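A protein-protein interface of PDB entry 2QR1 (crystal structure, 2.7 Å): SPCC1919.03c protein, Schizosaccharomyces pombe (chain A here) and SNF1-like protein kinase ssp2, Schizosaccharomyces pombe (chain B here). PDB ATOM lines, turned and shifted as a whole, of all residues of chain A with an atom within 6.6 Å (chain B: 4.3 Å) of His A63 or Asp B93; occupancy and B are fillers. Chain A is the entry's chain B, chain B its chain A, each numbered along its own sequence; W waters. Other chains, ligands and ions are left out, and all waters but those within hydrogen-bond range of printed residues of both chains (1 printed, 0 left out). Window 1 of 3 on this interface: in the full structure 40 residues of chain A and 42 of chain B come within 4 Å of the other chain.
His A63 touches just these residues of chain B: Phe B15, Asp B93, Val B94 and Lys B95. Asp B93 touches one residue of chain A. Printed residues of chain A within 4 Å of Phe B15: Leu A35 (3.7 Å), Leu A60 (3.9 Å), His A63 (3.6 Å), Leu A64 (3.6 Å) and Ala A65 (3.9 Å). Of the printed residues of chain B, Ala A65 touches Phe B15 (3.9 Å). Printed residues of chain A within 4 Å of Tyr B83: Leu A35 (3.9 Å). Leu B92 touches none of the printed residues of chain A. The nearest printed residue of chain B that does not touch His A63 is Glu B79 (6.0 Å). The nearest residue of chain A that does not touch Asp B93 is Leu A35 (4.2 Å).
Water W1 lies within hydrogen-bond range of the side-chain carboxylate of Asp B93, the backbone carbonyl oxygen of Leu A64 and the backbone NH of Val B94.
The backbone carbonyl oxygen (O) of Val B94 sits at hydrogen-bond distance from the backbone NH (N) of Leu A64 (2.8 Å). The side-chain carboxylate (OD1) of Asp B93 lies within hydrogen-bond range of a ring nitrogen (ND1) of His A63 (2.6 Å).
A ring nitrogen (NE2) of His A63 sits at hydrogen-bond distance from the backbone carbonyl oxygen (O) of Val A59 (3.5 Å). O of Gln B81 is in hydrogen-bond range of N of Asp B93, 2.7 Å away. The backbone carbonyl oxygen (O) of Glu B79 lies within hydrogen-bond range of the backbone NH (N) of Lys B95, 2.9 Å away. N of Asn A62 is in hydrogen-bond range of O of Thr A79 (2.8 Å). The backbone NH of Tyr B83 lies within hydrogen-bond range of the backbone carbonyl oxygen of Met B91. The backbone carbonyl oxygen (O) of Ser A77 is in hydrogen-bond range of the backbone NH (N) of Ala A65 (2.9 Å).
Leu A35 touches Phe B15 (O to CD1, 3.7 Å). Tyr B83 touches Leu A35 (CE2 to CD1, 3.9 Å). CE of Met B91 touches O of Leu A35, 3.8 Å away. Phe B15 touches Leu A60. Lys B95 touches Asn A62 (CA to O, 3.3 Å). His A63 touches Phe B15. His A63 touches Val B94. CB of Lys B95 touches CD2 of His A63, at 3.7 Å. O of Leu A64 touches CD2 of Phe B15 (3.6 Å). CA of Ala A65 touches CA of Phe B15, at 3.9 Å.
Of the 12 printed residues of chain A, 6 touch a printed residue of chain B. Printed residues of chain A that touch a printed residue of chain B: Leu A35, Leu A60, Asn A62, His A63, Leu A64 and Ala A65. Hydrophobic or aromatic side chains of chain A that line the printed part of chain B: Leu A35, Leu A60, His A63 and Leu A64. Of the 10 printed residues of chain B, 6 touch a printed residue of chain A. Among the printed residues, 13 pairs touch across the chains. Among the printed residues, no Asp or Glu carboxylate lies within 4 Å of a Lys or Arg side-chain nitrogen of the other chain.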
ATOM      1  N   HIS A  34      23.923   1.883  -2.593  1.00  0.00           N
ATOM      2  CA  HIS A  34      25.142   1.066  -2.518  1.00  0.00           C
ATOM      3  C   HIS A  34      25.034  -0.410  -2.989  1.00  0.00           C
ATOM      4  O   HIS A  34      26.055  -1.020  -3.304  1.00  0.00           O
ATOM      5  CB  HIS A  34      25.870   1.218  -1.161  1.00  0.00           C
ATOM      6  CG  HIS A  34      25.038   0.868   0.036  1.00  0.00           C
ATOM      7  ND1 HIS A  34      24.102   1.727   0.575  1.00  0.00           N
ATOM      8  CD2 HIS A  34      25.026  -0.237   0.819  1.00  0.00           C
ATOM      9  CE1 HIS A  34      23.533   1.154   1.624  1.00  0.00           C
ATOM     10  NE2 HIS A  34      24.077  -0.039   1.793  1.00  0.00           N
ATOM     11  N   LEU A  35      23.828  -0.976  -3.080  1.00  0.00           N
ATOM     12  CA  LEU A  35      23.687  -2.366  -3.565  1.00  0.00           C
ATOM     13  C   LEU A  35      23.440  -2.438  -5.064  1.00  0.00           C
ATOM     14  O   LEU A  35      23.072  -3.469  -5.609  1.00  0.00           O
ATOM     15  CB  LEU A  35      22.590  -3.119  -2.803  1.00  0.00           C
ATOM     16  CG  LEU A  35      22.779  -3.241  -1.292  1.00  0.00           C
ATOM     17  CD1 LEU A  35      21.458  -3.554  -0.615  1.00  0.00           C
ATOM     18  CD2 LEU A  35      23.826  -4.284  -0.943  1.00  0.00           C
ATOM     19  N   VAL A  59      30.354  -1.716   4.496  1.00  0.00           N
ATOM     20  CA  VAL A  59      28.941  -1.967   4.751  1.00  0.00           C
ATOM     21  C   VAL A  59      28.497  -3.293   4.140  1.00  0.00           C
ATOM     22  O   VAL A  59      27.480  -3.860   4.537  1.00  0.00           O
ATOM     23  CB  VAL A  59      28.057  -0.836   4.194  1.00  0.00           C
ATOM     24  CG1 VAL A  59      27.630   0.103   5.312  1.00  0.00           C
ATOM     25  CG2 VAL A  59      28.795  -0.075   3.103  1.00  0.00           C
ATOM     26  N   LEU A  60      29.268  -3.780   3.173  1.00  0.00           N
ATOM     27  CA  LEU A  60      28.764  -4.742   2.204  1.00  0.00           C
ATOM     28  C   LEU A  60      29.557  -6.024   2.381  1.00  0.00           C
ATOM     29  O   LEU A  60      29.323  -7.031   1.706  1.00  0.00           O
ATOM     30  CB  LEU A  60      28.740  -4.267   0.755  1.00  0.00           C
ATOM     31  CG  LEU A  60      27.902  -3.003   0.520  1.00  0.00           C
ATOM     32  CD1 LEU A  60      27.761  -2.678  -0.968  1.00  0.00           C
ATOM     33  CD2 LEU A  60      26.526  -3.128   1.172  1.00  0.00           C
ATOM     34  N   LEU A  61      30.490  -6.000   3.312  1.00  0.00           N
ATOM     35  CA  LEU A  61      31.072  -7.229   3.787  1.00  0.00           C
ATOM     36  C   LEU A  61      29.965  -8.236   4.151  1.00  0.00           C
ATOM     37  O   LEU A  61      29.039  -7.912   4.882  1.00  0.00           O
ATOM     38  CB  LEU A  61      31.931  -6.922   4.997  1.00  0.00           C
ATOM     39  CG  LEU A  61      33.422  -6.620   4.801  1.00  0.00           C
ATOM     40  CD1 LEU A  61      33.825  -6.336   3.371  1.00  0.00           C
ATOM     41  CD2 LEU A  61      33.818  -5.495   5.720  1.00  0.00           C
ATOM     42  N   ASN A  62      30.042  -9.438   3.595  1.00  0.00           N
ATOM     43  CA  ASN A  62      29.148 -10.541   3.948  1.00  0.00           C
ATOM     44  C   ASN A  62      27.750 -10.546   3.352  1.00  0.00           C
ATOM     45  O   ASN A  62      26.907 -11.347   3.750  1.00  0.00           O
ATOM     46  CB  ASN A  62      29.084 -10.697   5.461  1.00  0.00           C
ATOM     47  CG  ASN A  62      30.424 -11.100   6.053  1.00  0.00           C
ATOM     48  OD1 ASN A  62      30.828 -10.571   7.127  1.00  0.00           O
ATOM     49  ND2 ASN A  62      31.135 -12.047   5.365  1.00  0.00           N
ATOM     50  N   HIS A  63      27.500  -9.659   2.400  1.00  0.00           N
ATOM     51  CA  HIS A  63      26.257  -9.698   1.633  1.00  0.00           C
ATOM     52  C   HIS A  63      26.417 -10.654   0.456  1.00  0.00           C
ATOM     53  O   HIS A  63      27.310 -10.485  -0.373  1.00  0.00           O
ATOM     54  CB  HIS A  63      25.893  -8.298   1.121  1.00  0.00           C
ATOM     55  CG  HIS A  63      25.334  -7.380   2.165  1.00  0.00           C
ATOM     56  ND1 HIS A  63      24.080  -6.809   2.058  1.00  0.00           N
ATOM     57  CD2 HIS A  63      25.859  -6.911   3.322  1.00  0.00           C
ATOM     58  CE1 HIS A  63      23.856  -6.039   3.106  1.00  0.00           C
ATOM     59  NE2 HIS A  63      24.917  -6.086   3.891  1.00  0.00           N
ATOM     60  N   LEU A  64      25.559 -11.653   0.362  1.00  0.00           N
ATOM     61  CA  LEU A  64      25.596 -12.546  -0.787  1.00  0.00           C
ATOM     62  C   LEU A  64      25.308 -11.788  -2.083  1.00  0.00           C
ATOM     63  O   LEU A  64      24.445 -10.909  -2.116  1.00  0.00           O
ATOM     64  CB  LEU A  64      24.591 -13.670  -0.603  1.00  0.00           C
ATOM     65  CG  LEU A  64      24.193 -14.518  -1.815  1.00  0.00           C
ATOM     66  CD1 LEU A  64      25.358 -15.396  -2.373  1.00  0.00           C
ATOM     67  CD2 LEU A  64      22.994 -15.371  -1.430  1.00  0.00           C
ATOM     68  N   ALA A  65      26.062 -12.112  -3.131  1.00  0.00           N
ATOM     69  CA  ALA A  65      25.781 -11.663  -4.486  1.00  0.00           C
ATOM     70  C   ALA A  65      25.644 -12.909  -5.337  1.00  0.00           C
ATOM     71  O   ALA A  65      26.133 -13.973  -4.954  1.00  0.00           O
ATOM     72  CB  ALA A  65      26.903 -10.809  -5.000  1.00  0.00           C
ATOM     73  N   SER A  77      28.786 -15.424  -4.214  1.00  0.00           N
ATOM     74  CA  SER A  77      29.958 -14.835  -3.600  1.00  0.00           C
ATOM     75  C   SER A  77      29.658 -13.912  -2.463  1.00  0.00           C
ATOM     76  O   SER A  77      28.591 -13.297  -2.421  1.00  0.00           O
ATOM     77  CB  SER A  77      30.795 -14.080  -4.623  1.00  0.00           C
ATOM     78  OG  SER A  77      29.968 -13.246  -5.395  1.00  0.00           O
ATOM     79  N   ALA A  78      30.620 -13.824  -1.548  1.00  0.00           N
ATOM     80  CA  ALA A  78      30.603 -12.801  -0.500  1.00  0.00           C
ATOM     81  C   ALA A  78      32.012 -12.210  -0.285  1.00  0.00           C
ATOM     82  O   ALA A  78      33.010 -12.830  -0.640  1.00  0.00           O
ATOM     83  CB  ALA A  78      30.059 -13.392   0.789  1.00  0.00           C
ATOM     84  N   THR A  79      32.099 -11.022   0.291  1.00  0.00           N
ATOM     85  CA  THR A  79      33.397 -10.441   0.595  1.00  0.00           C
ATOM     86  C   THR A  79      33.570 -10.416   2.088  1.00  0.00           C
ATOM     87  O   THR A  79      32.617 -10.136   2.797  1.00  0.00           O
ATOM     88  CB  THR A  79      33.505  -9.023   0.055  1.00  0.00           C
ATOM     89  OG1 THR A  79      33.364  -9.064  -1.368  1.00  0.00           O
ATOM     90  CG2 THR A  79      34.844  -8.432   0.393  1.00  0.00           C
ATOM     91  N   PHE B  15      23.876  -8.018  -6.095  1.00  0.00           N
ATOM     92  CA  PHE B  15      23.580  -8.447  -4.756  1.00  0.00           C
ATOM     93  C   PHE B  15      22.252  -9.151  -4.687  1.00  0.00           C
ATOM     94  O   PHE B  15      21.347  -8.850  -5.456  1.00  0.00           O
ATOM     95  CB  PHE B  15      23.617  -7.273  -3.821  1.00  0.00           C
ATOM     96  CG  PHE B  15      25.012  -6.855  -3.458  1.00  0.00           C
ATOM     97  CD1 PHE B  15      25.605  -5.751  -4.062  1.00  0.00           C
ATOM     98  CD2 PHE B  15      25.740  -7.573  -2.509  1.00  0.00           C
ATOM     99  CE1 PHE B  15      26.881  -5.373  -3.736  1.00  0.00           C
ATOM    100  CE2 PHE B  15      27.026  -7.201  -2.163  1.00  0.00           C
ATOM    101  CZ  PHE B  15      27.600  -6.103  -2.782  1.00  0.00           C
ATOM    102  N   GLU B  79      20.564 -12.583   8.073  1.00  0.00           N
ATOM    103  CA  GLU B  79      19.518 -11.576   7.911  1.00  0.00           C
ATOM    104  C   GLU B  79      19.130 -11.425   6.438  1.00  0.00           C
ATOM    105  O   GLU B  79      19.991 -11.283   5.579  1.00  0.00           O
ATOM    106  CB  GLU B  79      19.986 -10.242   8.451  1.00  0.00           C
ATOM    107  CG  GLU B  79      19.064  -9.067   8.121  1.00  0.00           C
ATOM    108  CD  GLU B  79      19.612  -7.698   8.607  1.00  0.00           C
ATOM    109  OE1 GLU B  79      19.508  -7.431   9.828  1.00  0.00           O
ATOM    110  OE2 GLU B  79      20.133  -6.896   7.766  1.00  0.00           O
ATOM    111  N   LEU B  80      17.830 -11.475   6.155  1.00  0.00           N
ATOM    112  CA  LEU B  80      17.295 -11.258   4.809  1.00  0.00           C
ATOM    113  C   LEU B  80      16.579  -9.933   4.819  1.00  0.00           C
ATOM    114  O   LEU B  80      16.046  -9.525   5.831  1.00  0.00           O
ATOM    115  CB  LEU B  80      16.266 -12.324   4.419  1.00  0.00           C
ATOM    116  CG  LEU B  80      16.352 -13.845   4.670  1.00  0.00           C
ATOM    117  CD1 LEU B  80      17.168 -14.557   3.632  1.00  0.00           C
ATOM    118  CD2 LEU B  80      16.797 -14.201   6.064  1.00  0.00           C
ATOM    119  N   GLN B  81      16.556  -9.265   3.679  1.00  0.00           N
ATOM    120  CA  GLN B  81      15.845  -8.007   3.559  1.00  0.00           C
ATOM    121  C   GLN B  81      15.311  -7.835   2.155  1.00  0.00           C
ATOM    122  O   GLN B  81      16.063  -7.957   1.197  1.00  0.00           O
ATOM    123  CB  GLN B  81      16.783  -6.856   3.843  1.00  0.00           C
ATOM    124  CG  GLN B  81      16.140  -5.499   3.663  1.00  0.00           C
ATOM    125  CD  GLN B  81      15.445  -5.073   4.886  1.00  0.00           C
ATOM    126  OE1 GLN B  81      15.995  -5.162   5.983  1.00  0.00           O
ATOM    127  NE2 GLN B  81      14.223  -4.624   4.733  1.00  0.00           N
ATOM    128  N   TYR B  83      13.827  -5.364  -0.808  1.00  0.00           N
ATOM    129  CA  TYR B  83      13.823  -3.993  -1.286  1.00  0.00           C
ATOM    130  C   TYR B  83      13.064  -3.910  -2.594  1.00  0.00           C
ATOM    131  O   TYR B  83      13.342  -4.693  -3.486  1.00  0.00           O
ATOM    132  CB  TYR B  83      15.240  -3.517  -1.544  1.00  0.00           C
ATOM    133  CG  TYR B  83      16.098  -3.330  -0.323  1.00  0.00           C
ATOM    134  CD1 TYR B  83      15.893  -2.243   0.537  1.00  0.00           C
ATOM    135  CD2 TYR B  83      17.143  -4.212  -0.033  1.00  0.00           C
ATOM    136  CE1 TYR B  83      16.698  -2.059   1.665  1.00  0.00           C
ATOM    137  CE2 TYR B  83      17.954  -4.023   1.083  1.00  0.00           C
ATOM    138  CZ  TYR B  83      17.722  -2.950   1.917  1.00  0.00           C
ATOM    139  OH  TYR B  83      18.497  -2.759   3.020  1.00  0.00           O
ATOM    140  N   MET B  91      14.853  -6.968  -4.833  1.00  0.00           N
ATOM    141  CA  MET B  91      16.060  -7.663  -4.480  1.00  0.00           C
ATOM    142  C   MET B  91      15.784  -8.276  -3.130  1.00  0.00           C
ATOM    143  O   MET B  91      15.359  -7.597  -2.181  1.00  0.00           O
ATOM    144  CB  MET B  91      17.252  -6.699  -4.388  1.00  0.00           C
ATOM    145  CG  MET B  91      18.421  -7.246  -3.551  1.00  0.00           C
ATOM    146  SD  MET B  91      19.974  -6.304  -3.547  1.00  0.00           S
ATOM    147  CE  MET B  91      20.218  -5.881  -5.293  1.00  0.00           C
ATOM    148  N   LEU B  92      16.006  -9.568  -3.031  1.00  0.00           N
ATOM    149  CA  LEU B  92      15.993 -10.172  -1.734  1.00  0.00           C
ATOM    150  C   LEU B  92      17.440 -10.233  -1.268  1.00  0.00           C
ATOM    151  O   LEU B  92      18.208 -11.035  -1.787  1.00  0.00           O
ATOM    152  CB  LEU B  92      15.357 -11.553  -1.818  1.00  0.00           C
ATOM    153  CG  LEU B  92      15.689 -12.357  -0.578  1.00  0.00           C
ATOM    154  CD1 LEU B  92      14.770 -11.906   0.538  1.00  0.00           C
ATOM    155  CD2 LEU B  92      15.586 -13.838  -0.883  1.00  0.00           C
ATOM    156  N   ASP B  93      17.818  -9.370  -0.329  1.00  0.00           N
ATOM    157  CA  ASP B  93      19.225  -9.263   0.124  1.00  0.00           C
ATOM    158  C   ASP B  93      19.545 -10.180   1.321  1.00  0.00           C
ATOM    159  O   ASP B  93      18.783 -10.267   2.288  1.00  0.00           O
ATOM    160  CB  ASP B  93      19.631  -7.802   0.405  1.00  0.00           C
ATOM    161  CG  ASP B  93      20.932  -7.680   1.237  1.00  0.00           C
ATOM    162  OD1 ASP B  93      22.062  -7.709   0.645  1.00  0.00           O
ATOM    163  OD2 ASP B  93      20.809  -7.532   2.491  1.00  0.00           O
ATOM    164  N   VAL B  94      20.681 -10.855   1.230  1.00  0.00           N
ATOM    165  CA  VAL B  94      21.038 -11.851   2.188  1.00  0.00           C
ATOM    166  C   VAL B  94      22.383 -11.479   2.750  1.00  0.00           C
ATOM    167  O   VAL B  94      23.343 -11.359   1.997  1.00  0.00           O
ATOM    168  CB  VAL B  94      21.140 -13.252   1.531  1.00  0.00           C
ATOM    169  CG1 VAL B  94      21.659 -14.278   2.536  1.00  0.00           C
ATOM    170  CG2 VAL B  94      19.801 -13.690   1.019  1.00  0.00           C
ATOM    171  N   LYS B  95      22.456 -11.316   4.065  1.00  0.00           N
ATOM    172  CA  LYS B  95      23.733 -11.036   4.717  1.00  0.00           C
ATOM    173  C   LYS B  95      24.010 -11.854   6.002  1.00  0.00           C
ATOM    174  O   LYS B  95      23.093 -12.345   6.680  1.00  0.00           O
ATOM    175  CB  LYS B  95      23.903  -9.536   4.947  1.00  0.00           C
ATOM    176  CG  LYS B  95      23.321  -9.003   6.228  1.00  0.00           C
ATOM    177  CD  LYS B  95      24.448  -8.639   7.165  1.00  0.00           C
ATOM    178  CE  LYS B  95      24.049  -7.510   8.130  1.00  0.00           C
ATOM    179  NZ  LYS B  95      25.147  -7.201   9.101  1.00  0.00           N
HETATM  180  O   HOH W   1      22.609  -9.811  -0.634  1.00  0.00           O
